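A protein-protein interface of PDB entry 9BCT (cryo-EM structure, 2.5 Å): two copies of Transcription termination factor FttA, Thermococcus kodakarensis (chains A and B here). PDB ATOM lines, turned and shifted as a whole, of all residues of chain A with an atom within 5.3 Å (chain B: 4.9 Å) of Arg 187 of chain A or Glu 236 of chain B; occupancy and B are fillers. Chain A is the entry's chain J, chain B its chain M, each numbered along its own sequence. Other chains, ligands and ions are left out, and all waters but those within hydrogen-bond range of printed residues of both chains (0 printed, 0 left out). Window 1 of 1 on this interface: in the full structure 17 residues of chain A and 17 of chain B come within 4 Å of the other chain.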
ATOM      1  N   TRP A 185      -9.491   9.032  11.230  1.00  0.00           N
ATOM      2  CA  TRP A 185     -10.679   9.391  10.472  1.00  0.00           C
ATOM      3  C   TRP A 185     -11.220   8.156   9.769  1.00  0.00           C
ATOM      4  O   TRP A 185     -10.465   7.253   9.399  1.00  0.00           O
ATOM      5  CB  TRP A 185     -10.382  10.496   9.450  1.00  0.00           C
ATOM      6  CG  TRP A 185      -9.137  10.257   8.653  1.00  0.00           C
ATOM      7  CD1 TRP A 185      -7.874  10.663   8.965  1.00  0.00           C
ATOM      8  CD2 TRP A 185      -9.036   9.556   7.408  1.00  0.00           C
ATOM      9  NE1 TRP A 185      -6.992  10.259   7.994  1.00  0.00           N
ATOM     10  CE2 TRP A 185      -7.681   9.577   7.026  1.00  0.00           C
ATOM     11  CE3 TRP A 185      -9.961   8.913   6.580  1.00  0.00           C
ATOM     12  CZ2 TRP A 185      -7.227   8.980   5.852  1.00  0.00           C
ATOM     13  CZ3 TRP A 185      -9.508   8.321   5.415  1.00  0.00           C
ATOM     14  CH2 TRP A 185      -8.155   8.359   5.062  1.00  0.00           C
ATOM     15  N   ILE A 186     -12.537   8.129   9.590  1.00  0.00           N
ATOM     16  CA  ILE A 186     -13.231   7.055   8.890  1.00  0.00           C
ATOM     17  C   ILE A 186     -14.046   7.678   7.767  1.00  0.00           C
ATOM     18  O   ILE A 186     -14.789   8.639   7.995  1.00  0.00           O
ATOM     19  CB  ILE A 186     -14.132   6.245   9.840  1.00  0.00           C
ATOM     20  CG1 ILE A 186     -13.287   5.509  10.879  1.00  0.00           C
ATOM     21  CG2 ILE A 186     -14.994   5.266   9.059  1.00  0.00           C
ATOM     22  CD1 ILE A 186     -13.817   5.626  12.286  1.00  0.00           C
ATOM     23  N   ARG A 187     -13.907   7.135   6.560  1.00  0.00           N
ATOM     24  CA  ARG A 187     -14.561   7.688   5.385  1.00  0.00           C
ATOM     25  C   ARG A 187     -15.268   6.588   4.609  1.00  0.00           C
ATOM     26  O   ARG A 187     -14.768   5.465   4.510  1.00  0.00           O
ATOM     27  CB  ARG A 187     -13.553   8.390   4.479  1.00  0.00           C
ATOM     28  CG  ARG A 187     -14.046   9.699   3.910  1.00  0.00           C
ATOM     29  CD  ARG A 187     -12.878  10.571   3.516  1.00  0.00           C
ATOM     30  NE  ARG A 187     -12.034   9.918   2.525  1.00  0.00           N
ATOM     31  CZ  ARG A 187     -11.664  10.472   1.381  1.00  0.00           C
ATOM     32  NH1 ARG A 187     -12.046  11.695   1.049  1.00  0.00           N
ATOM     33  NH2 ARG A 187     -10.891   9.785   0.546  1.00  0.00           N
ATOM     34  N   ILE A 188     -16.429   6.927   4.055  1.00  0.00           N
ATOM     35  CA  ILE A 188     -17.204   6.028   3.207  1.00  0.00           C
ATOM     36  C   ILE A 188     -17.278   6.659   1.824  1.00  0.00           C
ATOM     37  O   ILE A 188     -17.693   7.817   1.687  1.00  0.00           O
ATOM     38  CB  ILE A 188     -18.607   5.772   3.781  1.00  0.00           C
ATOM     39  CG1 ILE A 188     -18.570   4.622   4.785  1.00  0.00           C
ATOM     40  CG2 ILE A 188     -19.603   5.448   2.675  1.00  0.00           C
ATOM     41  CD1 ILE A 188     -18.068   3.326   4.201  1.00  0.00           C
ATOM     42  N   THR A 189     -16.862   5.909   0.806  1.00  0.00           N
ATOM     43  CA  THR A 189     -16.872   6.389  -0.568  1.00  0.00           C
ATOM     44  C   THR A 189     -17.649   5.419  -1.444  1.00  0.00           C
ATOM     45  O   THR A 189     -17.530   4.200  -1.293  1.00  0.00           O
ATOM     46  CB  THR A 189     -15.452   6.557  -1.118  1.00  0.00           C
ATOM     47  OG1 THR A 189     -14.591   7.048  -0.083  1.00  0.00           O
ATOM     48  CG2 THR A 189     -15.445   7.533  -2.282  1.00  0.00           C
ATOM     49  N   LEU A 203     -16.197   1.806  -0.411  1.00  0.00           N
ATOM     50  CA  LEU A 203     -14.820   1.899   0.059  1.00  0.00           C
ATOM     51  C   LEU A 203     -14.820   2.500   1.455  1.00  0.00           C
ATOM     52  O   LEU A 203     -15.240   3.648   1.638  1.00  0.00           O
ATOM     53  CB  LEU A 203     -13.969   2.743  -0.894  1.00  0.00           C
ATOM     54  CG  LEU A 203     -12.456   2.506  -0.869  1.00  0.00           C
ATOM     55  CD1 LEU A 203     -12.138   1.023  -0.932  1.00  0.00           C
ATOM     56  CD2 LEU A 203     -11.782   3.246  -2.012  1.00  0.00           C
ATOM     57  N   VAL A 204     -14.357   1.726   2.431  1.00  0.00           N
ATOM     58  CA  VAL A 204     -14.173   2.193   3.798  1.00  0.00           C
ATOM     59  C   VAL A 204     -12.700   2.534   3.963  1.00  0.00           C
ATOM     60  O   VAL A 204     -11.835   1.656   3.853  1.00  0.00           O
ATOM     61  CB  VAL A 204     -14.615   1.135   4.821  1.00  0.00           C
ATOM     62  CG1 VAL A 204     -14.855   1.777   6.178  1.00  0.00           C
ATOM     63  CG2 VAL A 204     -15.857   0.408   4.332  1.00  0.00           C
ATOM     64  N   GLN A 205     -12.412   3.805   4.223  1.00  0.00           N
ATOM     65  CA  GLN A 205     -11.047   4.307   4.260  1.00  0.00           C
ATOM     66  C   GLN A 205     -10.715   4.813   5.654  1.00  0.00           C
ATOM     67  O   GLN A 205     -11.492   5.567   6.249  1.00  0.00           O
ATOM     68  CB  GLN A 205     -10.847   5.426   3.235  1.00  0.00           C
ATOM     69  CG  GLN A 205     -11.279   5.064   1.828  1.00  0.00           C
ATOM     70  CD  GLN A 205     -11.707   6.274   1.028  1.00  0.00           C
ATOM     71  OE1 GLN A 205     -11.558   7.410   1.475  1.00  0.00           O
ATOM     72  NE2 GLN A 205     -12.242   6.039  -0.163  1.00  0.00           N
ATOM     73  N   THR A 206      -9.568   4.392   6.167  1.00  0.00           N
ATOM     74  CA  THR A 206      -8.995   4.906   7.401  1.00  0.00           C
ATOM     75  C   THR A 206      -7.580   5.396   7.117  1.00  0.00           C
ATOM     76  O   THR A 206      -7.102   5.360   5.980  1.00  0.00           O
ATOM     77  CB  THR A 206      -8.996   3.836   8.498  1.00  0.00           C
ATOM     78  OG1 THR A 206      -8.301   2.672   8.033  1.00  0.00           O
ATOM     79  CG2 THR A 206     -10.419   3.456   8.876  1.00  0.00           C
ATOM     80  N   PRO A 235      -9.621   8.932  -7.507  1.00  0.00           N
ATOM     81  CA  PRO A 235      -8.237   9.018  -7.006  1.00  0.00           C
ATOM     82  C   PRO A 235      -7.977   8.147  -5.789  1.00  0.00           C
ATOM     83  O   PRO A 235      -6.876   7.598  -5.652  1.00  0.00           O
ATOM     84  CB  PRO A 235      -8.076  10.511  -6.686  1.00  0.00           C
ATOM     85  CG  PRO A 235      -9.110  11.197  -7.516  1.00  0.00           C
ATOM     86  CD  PRO A 235     -10.268  10.252  -7.585  1.00  0.00           C
ATOM     87  N   GLU A 236      -8.964   7.995  -4.902  1.00  0.00           N
ATOM     88  CA  GLU A 236      -8.786   7.121  -3.747  1.00  0.00           C
ATOM     89  C   GLU A 236      -8.664   5.662  -4.170  1.00  0.00           C
ATOM     90  O   GLU A 236      -7.790   4.939  -3.678  1.00  0.00           O
ATOM     91  CB  GLU A 236      -9.938   7.303  -2.757  1.00  0.00           C
ATOM     92  CG  GLU A 236     -11.326   7.373  -3.379  1.00  0.00           C
ATOM     93  CD  GLU A 236     -11.739   8.786  -3.745  1.00  0.00           C
ATOM     94  OE1 GLU A 236     -10.965   9.476  -4.438  1.00  0.00           O
ATOM     95  OE2 GLU A 236     -12.838   9.208  -3.330  1.00  0.00           O
ATOM     96  N   ALA A 644     -17.475  11.187  -0.881  1.00  0.00           N
ATOM     97  CA  ALA A 644     -16.863  10.711   0.352  1.00  0.00           C
ATOM     98  C   ALA A 644     -17.530  11.383   1.542  1.00  0.00           C
ATOM     99  O   ALA A 644     -17.645  12.613   1.585  1.00  0.00           O
ATOM    100  CB  ALA A 644     -15.358  10.984   0.362  1.00  0.00           C
ATOM    101  N   ILE A 645     -17.966  10.574   2.502  1.00  0.00           N
ATOM    102  CA  ILE A 645     -18.587  11.051   3.731  1.00  0.00           C
ATOM    103  C   ILE A 645     -17.670  10.678   4.886  1.00  0.00           C
ATOM    104  O   ILE A 645     -17.317   9.504   5.053  1.00  0.00           O
ATOM    105  CB  ILE A 645     -19.991  10.459   3.926  1.00  0.00           C
ATOM    106  CG1 ILE A 645     -20.835  10.659   2.666  1.00  0.00           C
ATOM    107  CG2 ILE A 645     -20.671  11.086   5.133  1.00  0.00           C
ATOM    108  CD1 ILE A 645     -21.178   9.372   1.953  1.00  0.00           C
ATOM    109  N   ARG A 646     -17.280  11.674   5.677  1.00  0.00           N
ATOM    110  CA  ARG A 646     -16.393  11.465   6.819  1.00  0.00           C
ATOM    111  C   ARG A 646     -17.253  11.135   8.032  1.00  0.00           C
ATOM    112  O   ARG A 646     -17.867  12.019   8.633  1.00  0.00           O
ATOM    113  CB  ARG A 646     -15.526  12.694   7.062  1.00  0.00           C
ATOM    114  CG  ARG A 646     -14.221  12.400   7.780  1.00  0.00           C
ATOM    115  CD  ARG A 646     -14.278  12.849   9.230  1.00  0.00           C
ATOM    116  NE  ARG A 646     -12.961  12.843   9.854  1.00  0.00           N
ATOM    117  CZ  ARG A 646     -12.160  13.897   9.919  1.00  0.00           C
ATOM    118  NH1 ARG A 646     -12.510  15.065   9.405  1.00  0.00           N
ATOM    119  NH2 ARG A 646     -10.976  13.776  10.514  1.00  0.00           N
ATOM    120  N   LEU A 647     -17.301   9.851   8.390  1.00  0.00           N
ATOM    121  CA  LEU A 647     -18.129   9.428   9.514  1.00  0.00           C
ATOM    122  C   LEU A 647     -17.528   9.863  10.844  1.00  0.00           C
ATOM    123  O   LEU A 647     -18.242  10.364  11.720  1.00  0.00           O
ATOM    124  CB  LEU A 647     -18.321   7.912   9.479  1.00  0.00           C
ATOM    125  CG  LEU A 647     -18.773   7.326   8.139  1.00  0.00           C
ATOM    126  CD1 LEU A 647     -19.012   5.835   8.268  1.00  0.00           C
ATOM    127  CD2 LEU A 647     -20.025   8.026   7.634  1.00  0.00           C
ATOM    128  N   ARG B 187     -15.588  16.928  -8.505  1.00  0.00           N
ATOM    129  CA  ARG B 187     -15.767  16.834  -7.064  1.00  0.00           C
ATOM    130  C   ARG B 187     -14.786  17.771  -6.378  1.00  0.00           C
ATOM    131  O   ARG B 187     -13.788  18.193  -6.963  1.00  0.00           O
ATOM    132  CB  ARG B 187     -15.582  15.395  -6.562  1.00  0.00           C
ATOM    133  CG  ARG B 187     -14.147  15.021  -6.243  1.00  0.00           C
ATOM    134  CD  ARG B 187     -13.876  13.569  -6.583  1.00  0.00           C
ATOM    135  NE  ARG B 187     -14.374  12.668  -5.550  1.00  0.00           N
ATOM    136  CZ  ARG B 187     -13.623  11.798  -4.890  1.00  0.00           C
ATOM    137  NH1 ARG B 187     -12.326  11.683  -5.128  1.00  0.00           N
ATOM    138  NH2 ARG B 187     -14.187  11.023  -3.969  1.00  0.00           N
ATOM    139  N   THR B 189     -12.806  18.225  -2.498  1.00  0.00           N
ATOM    140  CA  THR B 189     -12.463  17.611  -1.226  1.00  0.00           C
ATOM    141  C   THR B 189     -11.735  18.619  -0.349  1.00  0.00           C
ATOM    142  O   THR B 189     -10.857  19.350  -0.822  1.00  0.00           O
ATOM    143  CB  THR B 189     -11.586  16.369  -1.423  1.00  0.00           C
ATOM    144  OG1 THR B 189     -12.048  15.631  -2.561  1.00  0.00           O
ATOM    145  CG2 THR B 189     -11.639  15.476  -0.192  1.00  0.00           C
ATOM    146  N   LEU B 191      -9.116  19.093   2.299  1.00  0.00           N
ATOM    147  CA  LEU B 191      -8.012  18.553   3.079  1.00  0.00           C
ATOM    148  C   LEU B 191      -7.748  19.366   4.336  1.00  0.00           C
ATOM    149  O   LEU B 191      -7.069  18.879   5.247  1.00  0.00           O
ATOM    150  CB  LEU B 191      -6.743  18.489   2.228  1.00  0.00           C
ATOM    151  CG  LEU B 191      -6.942  18.180   0.743  1.00  0.00           C
ATOM    152  CD1 LEU B 191      -5.699  18.547  -0.052  1.00  0.00           C
ATOM    153  CD2 LEU B 191      -7.297  16.715   0.543  1.00  0.00           C
ATOM    154  N   LEU B 203      -9.328  20.750  -2.850  1.00  0.00           N
ATOM    155  CA  LEU B 203      -8.866  19.944  -3.975  1.00  0.00           C
ATOM    156  C   LEU B 203     -10.031  19.725  -4.929  1.00  0.00           C
ATOM    157  O   LEU B 203     -10.983  19.013  -4.594  1.00  0.00           O
ATOM    158  CB  LEU B 203      -8.294  18.608  -3.498  1.00  0.00           C
ATOM    159  CG  LEU B 203      -7.581  17.761  -4.554  1.00  0.00           C
ATOM    160  CD1 LEU B 203      -6.396  18.512  -5.138  1.00  0.00           C
ATOM    161  CD2 LEU B 203      -7.139  16.432  -3.965  1.00  0.00           C
ATOM    162  N   GLN B 205     -11.191  17.947  -8.148  1.00  0.00           N
ATOM    163  CA  GLN B 205     -10.794  16.772  -8.906  1.00  0.00           C
ATOM    164  C   GLN B 205     -11.791  16.521 -10.028  1.00  0.00           C
ATOM    165  O   GLN B 205     -13.001  16.447  -9.790  1.00  0.00           O
ATOM    166  CB  GLN B 205     -10.704  15.540  -8.003  1.00  0.00           C
ATOM    167  CG  GLN B 205      -9.859  15.742  -6.761  1.00  0.00           C
ATOM    168  CD  GLN B 205     -10.618  15.435  -5.488  1.00  0.00           C
ATOM    169  OE1 GLN B 205     -10.877  14.274  -5.171  1.00  0.00           O
ATOM    170  NE2 GLN B 205     -10.984  16.476  -4.752  1.00  0.00           N
ATOM    171  N   ALA B 234      -4.809  12.029   2.919  1.00  0.00           N
ATOM    172  CA  ALA B 234      -5.967  11.829   2.055  1.00  0.00           C
ATOM    173  C   ALA B 234      -5.562  11.008   0.836  1.00  0.00           C
ATOM    174  O   ALA B 234      -4.536  11.304   0.211  1.00  0.00           O
ATOM    175  CB  ALA B 234      -6.550  13.170   1.621  1.00  0.00           C
ATOM    176  N   PRO B 235      -6.318   9.963   0.485  1.00  0.00           N
ATOM    177  CA  PRO B 235      -5.922   9.129  -0.665  1.00  0.00           C
ATOM    178  C   PRO B 235      -5.852   9.889  -1.979  1.00  0.00           C
ATOM    179  O   PRO B 235      -4.967   9.609  -2.797  1.00  0.00           O
ATOM    180  CB  PRO B 235      -7.004   8.040  -0.689  1.00  0.00           C
ATOM    181  CG  PRO B 235      -7.566   8.021   0.697  1.00  0.00           C
ATOM    182  CD  PRO B 235      -7.511   9.438   1.168  1.00  0.00           C
ATOM    183  N   GLU B 236      -6.754  10.848  -2.208  1.00  0.00           N
ATOM    184  CA  GLU B 236      -6.679  11.642  -3.433  1.00  0.00           C
ATOM    185  C   GLU B 236      -5.434  12.516  -3.447  1.00  0.00           C
ATOM    186  O   GLU B 236      -4.754  12.617  -4.475  1.00  0.00           O
ATOM    187  CB  GLU B 236      -7.929  12.507  -3.595  1.00  0.00           C
ATOM    188  CG  GLU B 236      -9.206  11.876  -3.093  1.00  0.00           C
ATOM    189  CD  GLU B 236      -9.532  12.283  -1.675  1.00  0.00           C
ATOM    190  OE1 GLU B 236     -10.275  11.542  -1.007  1.00  0.00           O
ATOM    191  OE2 GLU B 236      -9.045  13.344  -1.230  1.00  0.00           O
ATOM    192  N   PHE B 237      -5.120  13.156  -2.319  1.00  0.00           N
ATOM    193  CA  PHE B 237      -3.923  13.985  -2.248  1.00  0.00           C
ATOM    194  C   PHE B 237      -2.662  13.145  -2.408  1.00  0.00           C
ATOM    195  O   PHE B 237      -1.714  13.560  -3.085  1.00  0.00           O
ATOM    196  CB  PHE B 237      -3.893  14.755  -0.929  1.00  0.00           C
ATOM    197  CG  PHE B 237      -3.161  16.063  -1.008  1.00  0.00           C
ATOM    198  CD1 PHE B 237      -3.125  16.780  -2.192  1.00  0.00           C
ATOM    199  CD2 PHE B 237      -2.505  16.573   0.099  1.00  0.00           C
ATOM    200  CE1 PHE B 237      -2.451  17.984  -2.270  1.00  0.00           C
ATOM    201  CE2 PHE B 237      -1.830  17.777   0.028  1.00  0.00           C
ATOM    202  CZ  PHE B 237      -1.803  18.483  -1.158  1.00  0.00           C
ATOM    203  N   ARG B 238      -2.636  11.961  -1.792  1.00  0.00           N
ATOM    204  CA  ARG B 238      -1.490  11.070  -1.945  1.00  0.00           C
ATOM    205  C   ARG B 238      -1.329  10.620  -3.392  1.00  0.00           C
ATOM    206  O   ARG B 238      -0.211  10.589  -3.917  1.00  0.00           O
ATOM    207  CB  ARG B 238      -1.641   9.860  -1.023  1.00  0.00           C
ATOM    208  CG  ARG B 238      -1.255  10.123   0.420  1.00  0.00           C
ATOM    209  CD  ARG B 238       0.069   9.463   0.767  1.00  0.00           C
ATOM    210  NE  ARG B 238       0.460   9.720   2.149  1.00  0.00           N
ATOM    211  CZ  ARG B 238       0.043   9.010   3.188  1.00  0.00           C
ATOM    212  NH1 ARG B 238      -0.782   7.986   3.042  1.00  0.00           N
ATOM    213  NH2 ARG B 238       0.464   9.337   4.407  1.00  0.00           N
ATOM    214  N   TYR B 239      -2.436  10.273  -4.050  1.00  0.00           N
ATOM    215  CA  TYR B 239      -2.375   9.850  -5.446  1.00  0.00           C
ATOM    216  C   TYR B 239      -1.921  10.989  -6.352  1.00  0.00           C
ATOM    217  O   TYR B 239      -1.164  10.769  -7.303  1.00  0.00           O
ATOM    218  CB  TYR B 239      -3.738   9.318  -5.889  1.00  0.00           C
ATOM    219  CG  TYR B 239      -3.850   9.053  -7.372  1.00  0.00           C
ATOM    220  CD1 TYR B 239      -3.131   8.027  -7.969  1.00  0.00           C
ATOM    221  CD2 TYR B 239      -4.678   9.825  -8.174  1.00  0.00           C
ATOM    222  CE1 TYR B 239      -3.231   7.779  -9.325  1.00  0.00           C
ATOM    223  CE2 TYR B 239      -4.787   9.586  -9.530  1.00  0.00           C
ATOM    224  CZ  TYR B 239      -4.060   8.562 -10.101  1.00  0.00           C
ATOM    225  OH  TYR B 239      -4.164   8.320 -11.450  1.00  0.00           O
ATOM    226  N   VAL B 240      -2.380  12.211  -6.076  1.00  0.00           N
ATOM    227  CA  VAL B 240      -2.003  13.356  -6.898  1.00  0.00           C
ATOM    228  C   VAL B 240      -0.527  13.688  -6.713  1.00  0.00           C
ATOM    229  O   VAL B 240       0.206  13.896  -7.688  1.00  0.00           O
ATOM    230  CB  VAL B 240      -2.904  14.562  -6.572  1.00  0.00           C
ATOM    231  CG1 VAL B 240      -2.259  15.856  -7.032  1.00  0.00           C
ATOM    232  CG2 VAL B 240      -4.271  14.387  -7.214  1.00  0.00           C
ATOM    233  N   LEU B 642     -11.950  16.127   4.915  1.00  0.00           N
ATOM    234  CA  LEU B 642     -11.969  14.908   4.104  1.00  0.00           C
ATOM    235  C   LEU B 642     -13.402  14.530   3.721  1.00  0.00           C
ATOM    236  O   LEU B 642     -13.935  13.494   4.122  1.00  0.00           O
ATOM    237  CB  LEU B 642     -11.260  13.752   4.821  1.00  0.00           C
ATOM    238  CG  LEU B 642      -9.785  13.966   5.161  1.00  0.00           C
ATOM    239  CD1 LEU B 642      -9.141  12.661   5.598  1.00  0.00           C
ATOM    240  CD2 LEU B 642      -9.048  14.561   3.975  1.00  0.00           C
ATOM    241  N   ASP B 643     -14.028  15.412   2.947  1.00  0.00           N
ATOM    242  CA  ASP B 643     -15.373  15.181   2.433  1.00  0.00           C
ATOM    243  C   ASP B 643     -15.403  15.580   0.968  1.00  0.00           C
ATOM    244  O   ASP B 643     -15.165  16.746   0.637  1.00  0.00           O
ATOM    245  CB  ASP B 643     -16.416  15.971   3.231  1.00  0.00           C
ATOM    246  CG  ASP B 643     -17.311  15.076   4.064  1.00  0.00           C
ATOM    247  OD1 ASP B 643     -16.932  13.911   4.303  1.00  0.00           O
ATOM    248  OD2 ASP B 643     -18.393  15.538   4.482  1.00  0.00           O
ATOM    249  N   ALA B 644     -15.695  14.621   0.097  1.00  0.00           N
ATOM    250  CA  ALA B 644     -15.764  14.859  -1.338  1.00  0.00           C
ATOM    251  C   ALA B 644     -17.222  15.029  -1.741  1.00  0.00           C
ATOM    252  O   ALA B 644     -18.051  14.153  -1.472  1.00  0.00           O
ATOM    253  CB  ALA B 644     -15.118  13.715  -2.117  1.00  0.00           C
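Arg 187 of chain A touches Pro 235 of chain B, and with the chains exchanged Pro 235 of chain A touches Arg 187 of chain B. Arg 187 of chain A touches Glu 236 of chain B, and with the chains exchanged Glu 236 of chain A touches Arg 187 of chain B. Pro 235 of chain B touches its own counterpart, Pro 235 of chain A. Ala 644 of chain B touches its own counterpart, Ala 644 of chain A. 7 positions are printed for both chains.
The side-chain carboxylate of Glu 236 of chain B is in salt-bridge range of the guanidinium group of Arg 187 of chain A (2.4 Å). The side-chain carboxylate (OE1) of Glu 236 of chain A is in salt-bridge range of the guanidinium group (NH1) of Arg 187 of chain B (2.7 Å). N of Ala 644 of chain A lies within hydrogen-bond range of O of Ala 644 of chain B (3.1 Å). The backbone NH of Arg 646 of chain A lies within hydrogen-bond range of the side-chain carboxylate of Asp 643 of chain B (2.6 Å). The backbone carbonyl oxygen of Ala 644 of chain A lies close to the side-chain carboxylate of Asp 643 of chain B, 3.1 Å away.
Hydrophobic or aromatic side chains of chain A that line the printed part of chain B: Trp 185, Pro 235 and Ala 644. Of the 15 printed residues of chain B, 7 touch a printed residue of chain A. Among the printed residues, Asp or Glu carboxylates within 4 Å of a Lys or Arg side-chain nitrogen of the other chain: Arg 187 of chain A with Glu 236 of chain B (2.4 Å) and Glu 236 of chain A with Arg 187 of chain B (2.3 Å).
Glu 236 of chain B touches just these residues of chain A: Arg 187, Pro 235 and Glu 236. Of the printed residues of chain B, Arg 646 of chain A touches Leu 642 (3.4 Å) and Asp 643 (2.6 Å). Of the printed residues of chain A, Tyr 239 of chain B touches Pro 235 (3.6 Å). Arg 238 of chain B touches none of the printed residues of chain A. Phe 237 of chain B touches none of the printed residues of chain A. The nearest residue of chain A that does not touch Glu 236 of chain B is Gln 205 of chain A (5.0 Å). The nearest printed residue of chain A that does not touch Pro 235 of chain B is Trp 185 of chain A (4.1 Å).
OE1 of Gln 205 of chain A lies within hydrogen-bond range of NH2 of Arg 187 of chain A. The backbone carbonyl oxygen (O) of Ile 188 of chain A lies within hydrogen-bond range of the backbone NH (N) of Ile 645 of chain A (2.9 Å). The backbone carbonyl oxygen of Arg 187 of chain B sits at hydrogen-bond distance from the backbone NH of Gln 205 of chain B (2.9 Å).
Pro 235 of chain B touches Arg 187 of chain A (CD to NH2, 3.5 Å). CD of Arg 187 of chain A touches O of Leu 642 of chain B, 3.2 Å away. Arg 187 of chain B touches Pro 235 of chain A (NH1 to CD, 3.5 Å). Pro 235 of chain A touches Pro 235 of chain B. CB of Pro 235 of chain A touches CB of Glu 236 of chain B (3.7 Å). CB of Tyr 239 of chain B touches O of Pro 235 of chain A, at 3.6 Å. Glu 236 of chain A touches Pro 235 of chain B (CA to CB, 3.7 Å). Glu 236 of chain A touches Glu 236 of chain B (OE1 to CG, 3.3 Å). Ile 645 of chain A touches Asp 643 of chain B (CA to OD1, 3.4 Å). CB of Arg 646 of chain A touches O of Leu 642 of chain B, 3.4 Å away.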
